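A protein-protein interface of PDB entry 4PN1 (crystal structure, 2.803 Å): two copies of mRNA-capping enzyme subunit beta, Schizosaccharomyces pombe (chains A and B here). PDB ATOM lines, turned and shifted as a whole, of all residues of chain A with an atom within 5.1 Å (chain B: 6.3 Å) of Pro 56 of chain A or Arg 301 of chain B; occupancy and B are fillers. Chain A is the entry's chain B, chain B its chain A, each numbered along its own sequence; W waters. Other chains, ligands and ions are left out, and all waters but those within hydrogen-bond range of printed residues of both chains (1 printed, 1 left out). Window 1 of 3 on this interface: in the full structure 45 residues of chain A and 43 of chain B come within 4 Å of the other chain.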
ATOM      1  N   ILE A  54     -14.023  28.982 -17.908  1.00  0.00           N
ATOM      2  CA  ILE A  54     -13.473  27.814 -18.585  1.00  0.00           C
ATOM      3  C   ILE A  54     -12.110  28.122 -19.196  1.00  0.00           C
ATOM      4  O   ILE A  54     -11.849  29.240 -19.644  1.00  0.00           O
ATOM      5  CB  ILE A  54     -14.428  27.251 -19.669  1.00  0.00           C
ATOM      6  CG1 ILE A  54     -14.523  28.201 -20.865  1.00  0.00           C
ATOM      7  CG2 ILE A  54     -15.810  26.975 -19.083  1.00  0.00           C
ATOM      8  CD1 ILE A  54     -15.192  27.589 -22.075  1.00  0.00           C
ATOM      9  N   VAL A  55     -11.237  27.121 -19.193  1.00  0.00           N
ATOM     10  CA  VAL A  55      -9.904  27.264 -19.753  1.00  0.00           C
ATOM     11  C   VAL A  55      -9.963  27.126 -21.266  1.00  0.00           C
ATOM     12  O   VAL A  55     -10.669  26.264 -21.785  1.00  0.00           O
ATOM     13  CB  VAL A  55      -8.961  26.179 -19.213  1.00  0.00           C
ATOM     14  CG1 VAL A  55      -7.525  26.682 -19.208  1.00  0.00           C
ATOM     15  CG2 VAL A  55      -9.389  25.759 -17.819  1.00  0.00           C
ATOM     16  N   PRO A  56      -9.234  27.991 -21.984  1.00  0.00           N
ATOM     17  CA  PRO A  56      -9.097  27.836 -23.436  1.00  0.00           C
ATOM     18  C   PRO A  56      -8.262  26.604 -23.780  1.00  0.00           C
ATOM     19  O   PRO A  56      -7.411  26.199 -22.986  1.00  0.00           O
ATOM     20  CB  PRO A  56      -8.354  29.109 -23.853  1.00  0.00           C
ATOM     21  CG  PRO A  56      -8.624  30.086 -22.761  1.00  0.00           C
ATOM     22  CD  PRO A  56      -8.674  29.267 -21.511  1.00  0.00           C
ATOM     23  N   ASP A  57      -8.510  26.020 -24.948  1.00  0.00           N
ATOM     24  CA  ASP A  57      -7.788  24.833 -25.398  1.00  0.00           C
ATOM     25  C   ASP A  57      -6.278  25.058 -25.423  1.00  0.00           C
ATOM     26  O   ASP A  57      -5.510  24.233 -24.926  1.00  0.00           O
ATOM     27  CB  ASP A  57      -8.264  24.427 -26.793  1.00  0.00           C
ATOM     28  CG  ASP A  57      -8.880  23.046 -26.820  1.00  0.00           C
ATOM     29  OD1 ASP A  57      -8.584  22.285 -27.767  1.00  0.00           O
ATOM     30  OD2 ASP A  57      -9.663  22.723 -25.903  1.00  0.00           O
ATOM     31  N   THR A  58      -5.869  26.180 -26.011  1.00  0.00           N
ATOM     32  CA  THR A  58      -4.460  26.539 -26.137  1.00  0.00           C
ATOM     33  C   THR A  58      -3.762  26.612 -24.780  1.00  0.00           C
ATOM     34  O   THR A  58      -2.663  26.084 -24.606  1.00  0.00           O
ATOM     35  CB  THR A  58      -4.296  27.885 -26.877  1.00  0.00           C
ATOM     36  OG1 THR A  58      -4.505  27.690 -28.283  1.00  0.00           O
ATOM     37  CG2 THR A  58      -2.909  28.462 -26.657  1.00  0.00           C
ATOM     38  N   THR A  59      -4.415  27.258 -23.820  1.00  0.00           N
ATOM     39  CA  THR A  59      -3.853  27.425 -22.485  1.00  0.00           C
ATOM     40  C   THR A  59      -3.702  26.085 -21.770  1.00  0.00           C
ATOM     41  O   THR A  59      -2.731  25.862 -21.046  1.00  0.00           O
ATOM     42  CB  THR A  59      -4.716  28.372 -21.637  1.00  0.00           C
ATOM     43  OG1 THR A  59      -4.892  29.606 -22.343  1.00  0.00           O
ATOM     44  CG2 THR A  59      -4.056  28.647 -20.290  1.00  0.00           C
ATOM     45  N   LYS A  60      -4.665  25.194 -21.984  1.00  0.00           N
ATOM     46  CA  LYS A  60      -4.620  23.860 -21.398  1.00  0.00           C
ATOM     47  C   LYS A  60      -3.438  23.065 -21.946  1.00  0.00           C
ATOM     48  O   LYS A  60      -2.688  22.447 -21.188  1.00  0.00           O
ATOM     49  CB  LYS A  60      -5.930  23.116 -21.666  1.00  0.00           C
ATOM     50  CG  LYS A  60      -5.979  21.697 -21.119  1.00  0.00           C
ATOM     51  CD  LYS A  60      -5.772  21.666 -19.613  1.00  0.00           C
ATOM     52  CE  LYS A  60      -6.237  20.343 -19.018  1.00  0.00           C
ATOM     53  NZ  LYS A  60      -5.669  19.171 -19.740  1.00  0.00           N
ATOM     54  N   GLN A 290      -1.881  31.889 -18.911  1.00  0.00           N
ATOM     55  CA  GLN A 290      -2.776  32.799 -19.617  1.00  0.00           C
ATOM     56  C   GLN A 290      -2.158  34.190 -19.692  1.00  0.00           C
ATOM     57  O   GLN A 290      -2.198  34.844 -20.735  1.00  0.00           O
ATOM     58  CB  GLN A 290      -4.129  32.881 -18.911  1.00  0.00           C
ATOM     59  CG  GLN A 290      -5.208  33.571 -19.720  1.00  0.00           C
ATOM     60  CD  GLN A 290      -5.624  32.755 -20.922  1.00  0.00           C
ATOM     61  OE1 GLN A 290      -5.717  31.529 -20.850  1.00  0.00           O
ATOM     62  NE2 GLN A 290      -5.868  33.429 -22.040  1.00  0.00           N
ATOM     63  N   ASP B 199     -11.459  17.096 -28.361  1.00  0.00           N
ATOM     64  CA  ASP B 199     -12.834  16.756 -28.016  1.00  0.00           C
ATOM     65  C   ASP B 199     -13.422  15.717 -28.966  1.00  0.00           C
ATOM     66  O   ASP B 199     -12.832  15.393 -29.999  1.00  0.00           O
ATOM     67  CB  ASP B 199     -13.704  18.014 -28.003  1.00  0.00           C
ATOM     68  CG  ASP B 199     -13.201  19.060 -27.024  1.00  0.00           C
ATOM     69  OD1 ASP B 199     -12.791  18.682 -25.905  1.00  0.00           O
ATOM     70  OD2 ASP B 199     -13.209  20.259 -27.376  1.00  0.00           O
ATOM     71  N   ALA B 200     -14.591  15.199 -28.609  1.00  0.00           N
ATOM     72  CA  ALA B 200     -15.243  14.167 -29.405  1.00  0.00           C
ATOM     73  C   ALA B 200     -16.023  14.761 -30.573  1.00  0.00           C
ATOM     74  O   ALA B 200     -16.405  14.044 -31.498  1.00  0.00           O
ATOM     75  CB  ALA B 200     -16.160  13.328 -28.529  1.00  0.00           C
ATOM     76  N   PHE B 201     -16.255  16.069 -30.529  1.00  0.00           N
ATOM     77  CA  PHE B 201     -17.054  16.733 -31.553  1.00  0.00           C
ATOM     78  C   PHE B 201     -16.282  17.824 -32.283  1.00  0.00           C
ATOM     79  O   PHE B 201     -15.287  18.339 -31.779  1.00  0.00           O
ATOM     80  CB  PHE B 201     -18.312  17.355 -30.938  1.00  0.00           C
ATOM     81  CG  PHE B 201     -19.178  16.380 -30.197  1.00  0.00           C
ATOM     82  CD1 PHE B 201     -19.040  16.215 -28.830  1.00  0.00           C
ATOM     83  CD2 PHE B 201     -20.138  15.638 -30.865  1.00  0.00           C
ATOM     84  CE1 PHE B 201     -19.837  15.323 -28.143  1.00  0.00           C
ATOM     85  CE2 PHE B 201     -20.939  14.743 -30.182  1.00  0.00           C
ATOM     86  CZ  PHE B 201     -20.787  14.586 -28.820  1.00  0.00           C
ATOM     87  N   VAL B 296     -20.702  26.858 -26.432  1.00  0.00           N
ATOM     88  CA  VAL B 296     -20.415  25.789 -27.381  1.00  0.00           C
ATOM     89  C   VAL B 296     -19.255  24.921 -26.899  1.00  0.00           C
ATOM     90  O   VAL B 296     -19.316  23.692 -26.963  1.00  0.00           O
ATOM     91  CB  VAL B 296     -20.099  26.354 -28.784  1.00  0.00           C
ATOM     92  CG1 VAL B 296     -19.571  25.265 -29.696  1.00  0.00           C
ATOM     93  CG2 VAL B 296     -21.338  26.990 -29.386  1.00  0.00           C
ATOM     94  N   ARG B 297     -18.204  25.567 -26.403  1.00  0.00           N
ATOM     95  CA  ARG B 297     -17.027  24.853 -25.919  1.00  0.00           C
ATOM     96  C   ARG B 297     -17.343  23.989 -24.699  1.00  0.00           C
ATOM     97  O   ARG B 297     -16.837  22.873 -24.576  1.00  0.00           O
ATOM     98  CB  ARG B 297     -15.889  25.831 -25.612  1.00  0.00           C
ATOM     99  CG  ARG B 297     -15.334  26.528 -26.846  1.00  0.00           C
ATOM    100  CD  ARG B 297     -14.184  27.460 -26.505  1.00  0.00           C
ATOM    101  NE  ARG B 297     -13.766  28.246 -27.664  1.00  0.00           N
ATOM    102  CZ  ARG B 297     -13.948  29.558 -27.785  1.00  0.00           C
ATOM    103  NH1 ARG B 297     -14.528  30.245 -26.810  1.00  0.00           N
ATOM    104  NH2 ARG B 297     -13.538  30.188 -28.878  1.00  0.00           N
ATOM    105  N   ILE B 298     -18.182  24.507 -23.806  1.00  0.00           N
ATOM    106  CA  ILE B 298     -18.606  23.758 -22.627  1.00  0.00           C
ATOM    107  C   ILE B 298     -19.290  22.455 -23.030  1.00  0.00           C
ATOM    108  O   ILE B 298     -18.955  21.384 -22.523  1.00  0.00           O
ATOM    109  CB  ILE B 298     -19.567  24.581 -21.747  1.00  0.00           C
ATOM    110  CG1 ILE B 298     -18.821  25.730 -21.071  1.00  0.00           C
ATOM    111  CG2 ILE B 298     -20.223  23.700 -20.691  1.00  0.00           C
ATOM    112  CD1 ILE B 298     -19.737  26.703 -20.376  1.00  0.00           C
ATOM    113  N   LEU B 299     -20.240  22.557 -23.954  1.00  0.00           N
ATOM    114  CA  LEU B 299     -20.978  21.395 -24.442  1.00  0.00           C
ATOM    115  C   LEU B 299     -20.090  20.423 -25.219  1.00  0.00           C
ATOM    116  O   LEU B 299     -20.288  19.211 -25.170  1.00  0.00           O
ATOM    117  CB  LEU B 299     -22.149  21.845 -25.318  1.00  0.00           C
ATOM    118  CG  LEU B 299     -23.251  22.604 -24.580  1.00  0.00           C
ATOM    119  CD1 LEU B 299     -24.242  23.210 -25.559  1.00  0.00           C
ATOM    120  CD2 LEU B 299     -23.955  21.678 -23.606  1.00  0.00           C
ATOM    121  N   ARG B 300     -19.110  20.967 -25.931  1.00  0.00           N
ATOM    122  CA  ARG B 300     -18.234  20.169 -26.781  1.00  0.00           C
ATOM    123  C   ARG B 300     -17.284  19.288 -25.967  1.00  0.00           C
ATOM    124  O   ARG B 300     -16.867  18.222 -26.421  1.00  0.00           O
ATOM    125  CB  ARG B 300     -17.435  21.090 -27.704  1.00  0.00           C
ATOM    126  CG  ARG B 300     -16.561  20.370 -28.710  1.00  0.00           C
ATOM    127  CD  ARG B 300     -15.726  21.358 -29.493  1.00  0.00           C
ATOM    128  NE  ARG B 300     -14.694  21.982 -28.669  1.00  0.00           N
ATOM    129  CZ  ARG B 300     -14.247  23.221 -28.846  1.00  0.00           C
ATOM    130  NH1 ARG B 300     -13.302  23.708 -28.053  1.00  0.00           N
ATOM    131  NH2 ARG B 300     -14.750  23.976 -29.812  1.00  0.00           N
ATOM    132  N   ARG B 301     -16.947  19.739 -24.764  1.00  0.00           N
ATOM    133  CA  ARG B 301     -16.015  19.015 -23.907  1.00  0.00           C
ATOM    134  C   ARG B 301     -16.727  17.954 -23.074  1.00  0.00           C
ATOM    135  O   ARG B 301     -16.102  17.017 -22.572  1.00  0.00           O
ATOM    136  CB  ARG B 301     -15.267  19.989 -22.995  1.00  0.00           C
ATOM    137  CG  ARG B 301     -14.447  21.017 -23.750  1.00  0.00           C
ATOM    138  CD  ARG B 301     -13.820  22.032 -22.816  1.00  0.00           C
ATOM    139  NE  ARG B 301     -13.126  23.081 -23.556  1.00  0.00           N
ATOM    140  CZ  ARG B 301     -12.456  24.079 -22.992  1.00  0.00           C
ATOM    141  NH1 ARG B 301     -12.385  24.172 -21.670  1.00  0.00           N
ATOM    142  NH2 ARG B 301     -11.856  24.987 -23.749  1.00  0.00           N
ATOM    143  N   GLU B 302     -18.039  18.104 -22.933  1.00  0.00           N
ATOM    144  CA  GLU B 302     -18.830  17.175 -22.140  1.00  0.00           C
ATOM    145  C   GLU B 302     -19.002  15.851 -22.874  1.00  0.00           C
ATOM    146  O   GLU B 302     -19.774  15.756 -23.828  1.00  0.00           O
ATOM    147  CB  GLU B 302     -20.196  17.780 -21.815  1.00  0.00           C
ATOM    148  CG  GLU B 302     -20.844  17.196 -20.575  1.00  0.00           C
ATOM    149  CD  GLU B 302     -20.054  17.492 -19.314  1.00  0.00           C
ATOM    150  OE1 GLU B 302     -19.470  18.593 -19.221  1.00  0.00           O
ATOM    151  OE2 GLU B 302     -20.014  16.623 -18.417  1.00  0.00           O
ATOM    152  N   HIS B 303     -18.271  14.835 -22.428  1.00  0.00           N
ATOM    153  CA  HIS B 303     -18.355  13.507 -23.020  1.00  0.00           C
ATOM    154  C   HIS B 303     -17.952  12.452 -21.993  1.00  0.00           C
ATOM    155  O   HIS B 303     -17.122  12.711 -21.121  1.00  0.00           O
ATOM    156  CB  HIS B 303     -17.461  13.413 -24.258  1.00  0.00           C
ATOM    157  CG  HIS B 303     -17.733  12.215 -25.112  1.00  0.00           C
ATOM    158  ND1 HIS B 303     -17.200  10.970 -24.845  1.00  0.00           N
ATOM    159  CD2 HIS B 303     -18.482  12.069 -26.232  1.00  0.00           C
ATOM    160  CE1 HIS B 303     -17.611  10.112 -25.761  1.00  0.00           C
ATOM    161  NE2 HIS B 303     -18.389  10.752 -26.613  1.00  0.00           N
ATOM    162  N   SER B 304     -18.544  11.267 -22.097  1.00  0.00           N
ATOM    163  CA  SER B 304     -18.276  10.188 -21.151  1.00  0.00           C
ATOM    164  C   SER B 304     -16.844   9.671 -21.259  1.00  0.00           C
ATOM    165  O   SER B 304     -16.293   9.560 -22.355  1.00  0.00           O
ATOM    166  CB  SER B 304     -19.267   9.041 -21.354  1.00  0.00           C
ATOM    167  OG  SER B 304     -19.190   8.528 -22.671  1.00  0.00           O
HETATM  168  O   HOH W   1     -12.031  22.194 -26.082  1.00  0.00           O
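NH2 of Arg 301 of chain B is in hydrogen-bond range of O of Val 55 of chain A (2.6 Å). NH2 of Arg 301 of chain B lies within salt-bridge range of OD2 of Asp 57 of chain A, 3.8 Å away.
Among the printed residues, pairs that only touch across the chains: Ile 54 of chain A with Ile 298 of chain B (3.8 Å) and Pro 56 of chain A with Arg 301 of chain B (3.9 Å).
Printed residues of chain B within 4 Å of Ile 54 of chain A: Ile 298 (3.8 Å). Of the printed residues of chain B, Val 55 of chain A touches Arg 301. Of chain B, only Arg 301 comes within 4 Å of Pro 56 of chain A. Of the printed residues of chain B, Asp 57 of chain A touches Arg 301. Of the printed residues of chain A, Arg 301 of chain B touches Val 55, Pro 56 and Asp 57. The nearest residue of chain B that does not touch Pro 56 of chain A is Arg 297 of chain B (6.0 Å). The nearest residue of chain A that does not touch Arg 301 of chain B is Ile 54 of chain A (4.2 Å). The nearest printed residue of chain A that does not touch Ile 298 of chain B is Val 55 of chain A (7.9 Å).
Printed residues of chain A that touch a printed residue of chain B: Ile 54, Val 55, Pro 56 and Asp 57. Hydrophobic or aromatic side chains of chain B that line the printed part of chain A: Ile 298. Along chain B the printed residues that touch a printed residue of chain A span positions 298 to 301.
No position is printed for both chains. Of the 4 pairs that touch across the chains among the printed residues, none has its exchanged pair printed and touching as well.
Water W1 lies within hydrogen-bond range of the side-chain carboxylate of Asp 57 of chain A (2.4 Å), the side-chain carboxylate of Asp 199 of chain B (2.6 Å), the guanidinium group of Arg 300 of chain B (2.8 Å) and the guanidinium group of Arg 301 of chain B (2.9 Å).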
